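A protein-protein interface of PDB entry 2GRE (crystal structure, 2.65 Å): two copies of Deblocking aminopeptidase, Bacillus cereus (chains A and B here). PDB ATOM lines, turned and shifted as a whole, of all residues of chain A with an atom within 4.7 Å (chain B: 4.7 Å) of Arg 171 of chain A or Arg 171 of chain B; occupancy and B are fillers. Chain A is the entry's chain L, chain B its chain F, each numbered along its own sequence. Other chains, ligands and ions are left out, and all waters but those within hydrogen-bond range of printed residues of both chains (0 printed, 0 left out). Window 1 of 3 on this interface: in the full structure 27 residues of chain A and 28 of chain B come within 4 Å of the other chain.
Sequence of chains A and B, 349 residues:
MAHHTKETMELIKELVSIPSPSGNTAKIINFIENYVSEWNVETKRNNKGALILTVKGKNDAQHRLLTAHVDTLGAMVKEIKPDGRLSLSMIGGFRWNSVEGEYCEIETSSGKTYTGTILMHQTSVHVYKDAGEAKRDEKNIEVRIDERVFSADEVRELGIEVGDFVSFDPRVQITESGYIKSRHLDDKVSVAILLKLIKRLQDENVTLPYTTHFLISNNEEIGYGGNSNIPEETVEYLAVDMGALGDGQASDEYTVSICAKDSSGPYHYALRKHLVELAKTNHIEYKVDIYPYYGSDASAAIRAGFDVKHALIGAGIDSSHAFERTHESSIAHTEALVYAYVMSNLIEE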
ATOM      1  N   GLY A 101      26.420  16.678 -33.949  1.00  0.00           N
ATOM      2  CA  GLY A 101      26.301  16.925 -32.523  1.00  0.00           C
ATOM      3  C   GLY A 101      25.270  17.959 -32.097  1.00  0.00           C
ATOM      4  O   GLY A 101      24.995  18.100 -30.915  1.00  0.00           O
ATOM      5  N   GLU A 102      24.688  18.692 -33.044  1.00  0.00           N
ATOM      6  CA  GLU A 102      23.726  19.690 -32.660  1.00  0.00           C
ATOM      7  C   GLU A 102      22.467  19.074 -32.108  1.00  0.00           C
ATOM      8  O   GLU A 102      22.103  17.946 -32.487  1.00  0.00           O
ATOM      9  CB  GLU A 102      23.376  20.572 -33.844  1.00  0.00           C
ATOM     10  CG  GLU A 102      24.233  21.828 -33.877  1.00  0.00           C
ATOM     11  CD  GLU A 102      23.984  22.895 -32.747  1.00  0.00           C
ATOM     12  OE1 GLU A 102      23.199  22.687 -31.760  1.00  0.00           O
ATOM     13  OE2 GLU A 102      24.636  23.965 -32.873  1.00  0.00           O
ATOM     14  N   TYR A 103      21.801  19.810 -31.209  1.00  0.00           N
ATOM     15  CA  TYR A 103      20.450  19.420 -30.779  1.00  0.00           C
ATOM     16  C   TYR A 103      19.433  19.901 -31.805  1.00  0.00           C
ATOM     17  O   TYR A 103      19.628  20.965 -32.443  1.00  0.00           O
ATOM     18  CB  TYR A 103      20.118  19.969 -29.425  1.00  0.00           C
ATOM     19  CG  TYR A 103      21.126  19.662 -28.367  1.00  0.00           C
ATOM     20  CD1 TYR A 103      21.253  20.510 -27.262  1.00  0.00           C
ATOM     21  CD2 TYR A 103      21.943  18.520 -28.433  1.00  0.00           C
ATOM     22  CE1 TYR A 103      22.160  20.252 -26.261  1.00  0.00           C
ATOM     23  CE2 TYR A 103      22.872  18.246 -27.422  1.00  0.00           C
ATOM     24  CZ  TYR A 103      22.973  19.125 -26.334  1.00  0.00           C
ATOM     25  OH  TYR A 103      23.886  18.923 -25.301  1.00  0.00           O
ATOM     26  N   ASP A 169      18.847  23.337 -33.558  1.00  0.00           N
ATOM     27  CA  ASP A 169      18.723  24.313 -32.512  1.00  0.00           C
ATOM     28  C   ASP A 169      19.675  25.458 -32.801  1.00  0.00           C
ATOM     29  O   ASP A 169      20.844  25.257 -33.023  1.00  0.00           O
ATOM     30  CB  ASP A 169      18.902  23.669 -31.142  1.00  0.00           C
ATOM     31  CG  ASP A 169      17.555  23.336 -30.492  1.00  0.00           C
ATOM     32  OD1 ASP A 169      17.170  22.150 -30.426  1.00  0.00           O
ATOM     33  OD2 ASP A 169      16.853  24.292 -30.084  1.00  0.00           O
ATOM     34  N   PRO A 170      19.154  26.670 -32.841  1.00  0.00           N
ATOM     35  CA  PRO A 170      19.939  27.783 -33.348  1.00  0.00           C
ATOM     36  C   PRO A 170      21.006  28.309 -32.394  1.00  0.00           C
ATOM     37  O   PRO A 170      21.902  29.020 -32.817  1.00  0.00           O
ATOM     38  CB  PRO A 170      18.892  28.859 -33.591  1.00  0.00           C
ATOM     39  CG  PRO A 170      17.746  28.513 -32.672  1.00  0.00           C
ATOM     40  CD  PRO A 170      17.803  27.056 -32.394  1.00  0.00           C
ATOM     41  N   ARG A 171      20.904  27.977 -31.112  1.00  0.00           N
ATOM     42  CA  ARG A 171      21.856  28.463 -30.108  1.00  0.00           C
ATOM     43  C   ARG A 171      22.162  29.961 -30.285  1.00  0.00           C
ATOM     44  O   ARG A 171      23.312  30.356 -30.449  1.00  0.00           O
ATOM     45  CB  ARG A 171      23.149  27.658 -30.190  1.00  0.00           C
ATOM     46  CG  ARG A 171      22.955  26.167 -30.254  1.00  0.00           C
ATOM     47  CD  ARG A 171      24.281  25.481 -29.941  1.00  0.00           C
ATOM     48  NE  ARG A 171      25.316  25.837 -30.915  1.00  0.00           N
ATOM     49  CZ  ARG A 171      26.627  25.807 -30.690  1.00  0.00           C
ATOM     50  NH1 ARG A 171      27.108  25.440 -29.505  1.00  0.00           N
ATOM     51  NH2 ARG A 171      27.454  26.163 -31.664  1.00  0.00           N
ATOM     52  N   VAL A 172      21.144  30.797 -30.273  1.00  0.00           N
ATOM     53  CA  VAL A 172      21.397  32.200 -30.559  1.00  0.00           C
ATOM     54  C   VAL A 172      21.888  32.971 -29.309  1.00  0.00           C
ATOM     55  O   VAL A 172      21.398  32.743 -28.197  1.00  0.00           O
ATOM     56  CB  VAL A 172      20.179  32.828 -31.262  1.00  0.00           C
ATOM     57  CG1 VAL A 172      18.919  32.675 -30.405  1.00  0.00           C
ATOM     58  CG2 VAL A 172      20.444  34.273 -31.630  1.00  0.00           C
ATOM     59  N   GLN A 173      22.902  33.817 -29.470  1.00  0.00           N
ATOM     60  CA  GLN A 173      23.422  34.599 -28.341  1.00  0.00           C
ATOM     61  C   GLN A 173      23.616  36.019 -28.788  1.00  0.00           C
ATOM     62  O   GLN A 173      24.072  36.264 -29.917  1.00  0.00           O
ATOM     63  CB  GLN A 173      24.731  34.040 -27.791  1.00  0.00           C
ATOM     64  CG  GLN A 173      24.567  32.787 -26.901  1.00  0.00           C
ATOM     65  CD  GLN A 173      25.863  32.349 -26.202  1.00  0.00           C
ATOM     66  OE1 GLN A 173      25.933  31.262 -25.649  1.00  0.00           O
ATOM     67  NE2 GLN A 173      26.879  33.197 -26.217  1.00  0.00           N
ATOM     68  N   LYS A 181      25.621  35.914 -32.210  1.00  0.00           N
ATOM     69  CA  LYS A 181      26.020  34.585 -32.693  1.00  0.00           C
ATOM     70  C   LYS A 181      24.796  33.765 -32.853  1.00  0.00           C
ATOM     71  O   LYS A 181      23.810  34.007 -32.163  1.00  0.00           O
ATOM     72  CB  LYS A 181      26.849  33.877 -31.662  1.00  0.00           C
ATOM     73  CG  LYS A 181      28.267  34.318 -31.649  1.00  0.00           C
ATOM     74  CD  LYS A 181      29.127  33.295 -30.953  1.00  0.00           C
ATOM     75  CE  LYS A 181      28.927  33.309 -29.463  1.00  0.00           C
ATOM     76  NZ  LYS A 181      30.078  32.623 -28.825  1.00  0.00           N
ATOM     77  N   SER A 182      24.835  32.793 -33.751  1.00  0.00           N
ATOM     78  CA  SER A 182      23.760  31.814 -33.838  1.00  0.00           C
ATOM     79  C   SER A 182      24.213  30.557 -34.588  1.00  0.00           C
ATOM     80  O   SER A 182      25.419  30.202 -34.598  1.00  0.00           O
ATOM     81  CB  SER A 182      22.516  32.431 -34.488  1.00  0.00           C
ATOM     82  OG  SER A 182      21.493  31.469 -34.658  1.00  0.00           O
ATOM     83  N   PHE A 323      28.559  28.504 -38.680  1.00  0.00           N
ATOM     84  CA  PHE A 323      28.259  29.148 -37.413  1.00  0.00           C
ATOM     85  C   PHE A 323      28.299  30.648 -37.589  1.00  0.00           C
ATOM     86  O   PHE A 323      29.353  31.241 -37.823  1.00  0.00           O
ATOM     87  CB  PHE A 323      29.235  28.639 -36.390  1.00  0.00           C
ATOM     88  CG  PHE A 323      29.524  27.165 -36.555  1.00  0.00           C
ATOM     89  CD1 PHE A 323      30.632  26.741 -37.287  1.00  0.00           C
ATOM     90  CD2 PHE A 323      28.655  26.214 -36.020  1.00  0.00           C
ATOM     91  CE1 PHE A 323      30.882  25.400 -37.458  1.00  0.00           C
ATOM     92  CE2 PHE A 323      28.895  24.867 -36.156  1.00  0.00           C
ATOM     93  CZ  PHE A 323      30.008  24.442 -36.880  1.00  0.00           C
ATOM     94  N   GLY B 101      32.549  24.636 -34.022  1.00  0.00           N
ATOM     95  CA  GLY B 101      31.395  25.474 -33.766  1.00  0.00           C
ATOM     96  C   GLY B 101      30.880  25.579 -32.339  1.00  0.00           C
ATOM     97  O   GLY B 101      29.805  26.143 -32.135  1.00  0.00           O
ATOM     98  N   GLU B 102      31.604  25.040 -31.356  1.00  0.00           N
ATOM     99  CA  GLU B 102      31.162  25.172 -29.983  1.00  0.00           C
ATOM    100  C   GLU B 102      31.493  26.573 -29.474  1.00  0.00           C
ATOM    101  O   GLU B 102      32.434  27.211 -29.962  1.00  0.00           O
ATOM    102  CB  GLU B 102      31.772  24.102 -29.110  1.00  0.00           C
ATOM    103  CG  GLU B 102      31.020  22.773 -29.143  1.00  0.00           C
ATOM    104  CD  GLU B 102      31.565  21.751 -28.096  1.00  0.00           C
ATOM    105  OE1 GLU B 102      31.445  20.497 -28.316  1.00  0.00           O
ATOM    106  OE2 GLU B 102      32.127  22.204 -27.052  1.00  0.00           O
ATOM    107  N   TYR B 103      30.683  27.069 -28.536  1.00  0.00           N
ATOM    108  CA  TYR B 103      30.939  28.360 -27.865  1.00  0.00           C
ATOM    109  C   TYR B 103      31.870  28.077 -26.715  1.00  0.00           C
ATOM    110  O   TYR B 103      31.780  27.004 -26.080  1.00  0.00           O
ATOM    111  CB  TYR B 103      29.655  29.030 -27.375  1.00  0.00           C
ATOM    112  CG  TYR B 103      28.713  29.419 -28.478  1.00  0.00           C
ATOM    113  CD1 TYR B 103      27.359  29.621 -28.224  1.00  0.00           C
ATOM    114  CD2 TYR B 103      29.166  29.541 -29.798  1.00  0.00           C
ATOM    115  CE1 TYR B 103      26.477  29.961 -29.243  1.00  0.00           C
ATOM    116  CE2 TYR B 103      28.297  29.875 -30.824  1.00  0.00           C
ATOM    117  CZ  TYR B 103      26.957  30.082 -30.540  1.00  0.00           C
ATOM    118  OH  TYR B 103      26.104  30.399 -31.564  1.00  0.00           O
ATOM    119  N   ASP B 169      31.475  25.265 -23.975  1.00  0.00           N
ATOM    120  CA  ASP B 169      30.189  25.421 -23.313  1.00  0.00           C
ATOM    121  C   ASP B 169      29.625  24.015 -23.247  1.00  0.00           C
ATOM    122  O   ASP B 169      29.613  23.314 -24.248  1.00  0.00           O
ATOM    123  CB  ASP B 169      29.264  26.400 -24.066  1.00  0.00           C
ATOM    124  CG  ASP B 169      29.594  27.892 -23.765  1.00  0.00           C
ATOM    125  OD1 ASP B 169      30.667  28.147 -23.159  1.00  0.00           O
ATOM    126  OD2 ASP B 169      28.788  28.811 -24.130  1.00  0.00           O
ATOM    127  N   PRO B 170      29.186  23.580 -22.068  1.00  0.00           N
ATOM    128  CA  PRO B 170      28.845  22.180 -21.951  1.00  0.00           C
ATOM    129  C   PRO B 170      27.442  21.823 -22.494  1.00  0.00           C
ATOM    130  O   PRO B 170      27.087  20.638 -22.538  1.00  0.00           O
ATOM    131  CB  PRO B 170      28.897  21.960 -20.438  1.00  0.00           C
ATOM    132  CG  PRO B 170      28.497  23.264 -19.863  1.00  0.00           C
ATOM    133  CD  PRO B 170      28.953  24.314 -20.809  1.00  0.00           C
ATOM    134  N   ARG B 171      26.652  22.828 -22.867  1.00  0.00           N
ATOM    135  CA  ARG B 171      25.267  22.631 -23.328  1.00  0.00           C
ATOM    136  C   ARG B 171      24.458  21.508 -22.634  1.00  0.00           C
ATOM    137  O   ARG B 171      23.828  20.675 -23.306  1.00  0.00           O
ATOM    138  CB  ARG B 171      25.240  22.479 -24.853  1.00  0.00           C
ATOM    139  CG  ARG B 171      25.613  23.787 -25.557  1.00  0.00           C
ATOM    140  CD  ARG B 171      25.395  23.717 -27.066  1.00  0.00           C
ATOM    141  NE  ARG B 171      25.861  22.425 -27.562  1.00  0.00           N
ATOM    142  CZ  ARG B 171      25.307  21.735 -28.555  1.00  0.00           C
ATOM    143  NH1 ARG B 171      24.240  22.198 -29.220  1.00  0.00           N
ATOM    144  NH2 ARG B 171      25.826  20.555 -28.861  1.00  0.00           N
ATOM    145  N   VAL B 172      24.458  21.503 -21.301  1.00  0.00           N
ATOM    146  CA  VAL B 172      23.774  20.453 -20.543  1.00  0.00           C
ATOM    147  C   VAL B 172      22.267  20.621 -20.540  1.00  0.00           C
ATOM    148  O   VAL B 172      21.770  21.741 -20.539  1.00  0.00           O
ATOM    149  CB  VAL B 172      24.284  20.358 -19.104  1.00  0.00           C
ATOM    150  CG1 VAL B 172      23.939  21.625 -18.339  1.00  0.00           C
ATOM    151  CG2 VAL B 172      23.714  19.102 -18.418  1.00  0.00           C
ATOM    152  N   GLN B 173      21.548  19.503 -20.549  1.00  0.00           N
ATOM    153  CA  GLN B 173      20.082  19.489 -20.606  1.00  0.00           C
ATOM    154  C   GLN B 173      19.607  18.199 -19.968  1.00  0.00           C
ATOM    155  O   GLN B 173      20.089  17.102 -20.338  1.00  0.00           O
ATOM    156  CB  GLN B 173      19.574  19.507 -22.034  1.00  0.00           C
ATOM    157  CG  GLN B 173      19.363  20.860 -22.653  1.00  0.00           C
ATOM    158  CD  GLN B 173      18.557  20.776 -23.954  1.00  0.00           C
ATOM    159  OE1 GLN B 173      18.731  21.603 -24.853  1.00  0.00           O
ATOM    160  NE2 GLN B 173      17.655  19.786 -24.053  1.00  0.00           N
ATOM    161  N   LYS B 181      21.921  15.153 -21.239  1.00  0.00           N
ATOM    162  CA  LYS B 181      22.741  15.336 -22.458  1.00  0.00           C
ATOM    163  C   LYS B 181      23.780  16.426 -22.221  1.00  0.00           C
ATOM    164  O   LYS B 181      23.497  17.434 -21.558  1.00  0.00           O
ATOM    165  CB  LYS B 181      21.867  15.890 -23.562  1.00  0.00           C
ATOM    166  CG  LYS B 181      21.378  14.965 -24.648  1.00  0.00           C
ATOM    167  CD  LYS B 181      20.903  15.786 -25.893  1.00  0.00           C
ATOM    168  CE  LYS B 181      19.610  16.586 -25.667  1.00  0.00           C
ATOM    169  NZ  LYS B 181      18.966  17.108 -26.972  1.00  0.00           N
ATOM    170  N   SER B 182      24.963  16.261 -22.804  1.00  0.00           N
ATOM    171  CA  SER B 182      25.958  17.328 -22.836  1.00  0.00           C
ATOM    172  C   SER B 182      26.916  17.210 -24.029  1.00  0.00           C
ATOM    173  O   SER B 182      26.576  16.682 -25.117  1.00  0.00           O
ATOM    174  CB  SER B 182      26.760  17.321 -21.532  1.00  0.00           C
ATOM    175  OG  SER B 182      27.709  18.380 -21.460  1.00  0.00           O
ATOM    176  N   ARG B 183      28.098  17.799 -23.818  1.00  0.00           N
ATOM    177  CA  ARG B 183      29.378  17.346 -24.391  1.00  0.00           C
ATOM    178  C   ARG B 183      30.320  17.617 -23.225  1.00  0.00           C
ATOM    179  O   ARG B 183      31.357  18.292 -23.361  1.00  0.00           O
ATOM    180  CB  ARG B 183      29.781  18.068 -25.685  1.00  0.00           C
ATOM    181  CG  ARG B 183      29.531  19.592 -25.697  1.00  0.00           C
ATOM    182  CD  ARG B 183      28.411  20.001 -26.656  1.00  0.00           C
ATOM    183  NE  ARG B 183      28.963  20.314 -27.991  1.00  0.00           N
ATOM    184  CZ  ARG B 183      28.703  19.662 -29.133  1.00  0.00           C
ATOM    185  NH1 ARG B 183      27.854  18.643 -29.132  1.00  0.00           N
ATOM    186  NH2 ARG B 183      29.288  20.040 -30.281  1.00  0.00           N
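Of the printed residues of chain B, Gly 101 of chain A touches Arg 171 (3.3 Å) and Arg 183 (3.4 Å).
Of the printed residues of chain B, Glu 102 of chain A touches Arg 171.
Pro 170 of chain A touches none of the printed residues of chain B.
Arg 171 of chain A touches just these residues of chain B: Gly 101, Tyr 103 and Arg 171.
Printed residues of chain B within 4 Å of Phe 323 of chain A: Gly 101.
Of the printed residues of chain A, Tyr 103 of chain B touches Arg 171, Gln 173, Lys 181 and Ser 182.
Of the printed residues of chain A, Arg 171 of chain B touches Gly 101 (3.3 Å), Glu 102 (2.8 Å), Tyr 103 (2.7 Å) and Arg 171 (3.4 Å).
Of the printed residues of chain A, Lys 181 of chain B touches Tyr 103 (3.5 Å).
The nearest residue of chain B that does not touch Arg 171 of chain A is Glu 102 of chain B (4.1 Å).
The nearest printed residue of chain A that does not touch Gln 173 of chain B is Asp 169 of chain A (5.8 Å).
NH2 of Arg 171 of chain B lies within hydrogen-bond range of O of Gly 101 of chain A (3.3 Å).
The guanidinium group (NH1) of Arg 183 of chain B sits at hydrogen-bond distance from the backbone carbonyl oxygen (O) of Gly 101 of chain A.
The guanidinium group of Arg 171 of chain B is in salt-bridge range of the side-chain carboxylate of Glu 102 of chain A (2.8 Å).
The guanidinium group of Arg 171 of chain A lies close to the backbone carbonyl oxygen of Gly 101 of chain B, at 2.4 Å.
O of Arg 171 of chain B sits at hydrogen-bond distance from OH of Tyr 103 of chain A (2.7 Å).
O of Ser 182 of chain A sits at hydrogen-bond distance from OH of Tyr 103 of chain B (3.1 Å).
The side-chain hydroxyl of Tyr 103 of chain B is in hydrogen-bond range of the backbone carbonyl oxygen of Arg 171 of chain A (3.0 Å).
The side-chain hydroxyl (OG) of Ser 182 of chain A sits at hydrogen-bond distance from the backbone carbonyl oxygen (O) of Pro 170 of chain A (3.1 Å).
The backbone carbonyl oxygen (O) of Tyr 103 of chain B lies within hydrogen-bond range of the backbone NH (N) of Asp 169 of chain B (2.7 Å).
The guanidinium group (NE) of Arg 183 of chain B is in salt-bridge range of the side-chain carboxylate (OE1) of Glu 102 of chain B (2.5 Å).
N of Lys 181 of chain A sits at hydrogen-bond distance from O of Gln 173 of chain A (2.8 Å).
The backbone carbonyl oxygen (O) of Tyr 103 of chain A lies within hydrogen-bond range of the backbone NH (N) of Asp 169 of chain A.
O of Gln 173 of chain B sits at hydrogen-bond distance from N of Lys 181 of chain B, at 2.8 Å.
Gln 173 of chain B touches Tyr 103 of chain A (OE1 to CD1, 3.7 Å).
Lys 181 of chain B touches Tyr 103 of chain A.
Tyr 103 of chain A touches Ser 182 of chain B.
CD of Arg 171 of chain A touches NH1 of Arg 171 of chain B, 3.4 Å away.
Gln 173 of chain A touches Tyr 103 of chain B (OE1 to CD1, 3.4 Å).
Lys 181 of chain A touches Tyr 103 of chain B (NZ to CD2, 3.4 Å).
Phe 323 of chain A touches Gly 101 of chain B.
Tyr 103 of chain A touches Arg 171 of chain B, and with the chains exchanged Arg 171 of chain A touches Tyr 103 of chain B.
Tyr 103 of chain A touches Gln 173 of chain B, and with the chains exchanged Gln 173 of chain A touches Tyr 103 of chain B.
Tyr 103 of chain A touches Lys 181 of chain B, and with the chains exchanged Lys 181 of chain A touches Tyr 103 of chain B.
Tyr 103 of chain A touches Ser 182 of chain B, and with the chains exchanged Ser 182 of chain A touches Tyr 103 of chain B.
10 positions are printed for both chains.
Of the 14 pairs that touch across the chains among the printed residues, 11 have their exchanged pair printed and touching as well.
Of the 11 printed residues of chain B, 7 touch a printed residue of chain A.
Printed residues of chain B that touch a printed residue of chain A: Gly 101, Tyr 103, Arg 171, Gln 173, Lys 181, Ser 182 and Arg 183.
Hydrophobic or aromatic side chains of chain B that line the printed part of chain A: Tyr 103.
Printed residues of chain A that touch a printed residue of chain B: Gly 101, Glu 102, Tyr 103, Arg 171, Gln 173, Lys 181, Ser 182 and Phe 323.
Hydrophobic or aromatic side chains of chain A that line the printed part of chain B: Tyr 103 and Phe 323.
Among the printed residues, 14 pairs touch across the chains.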
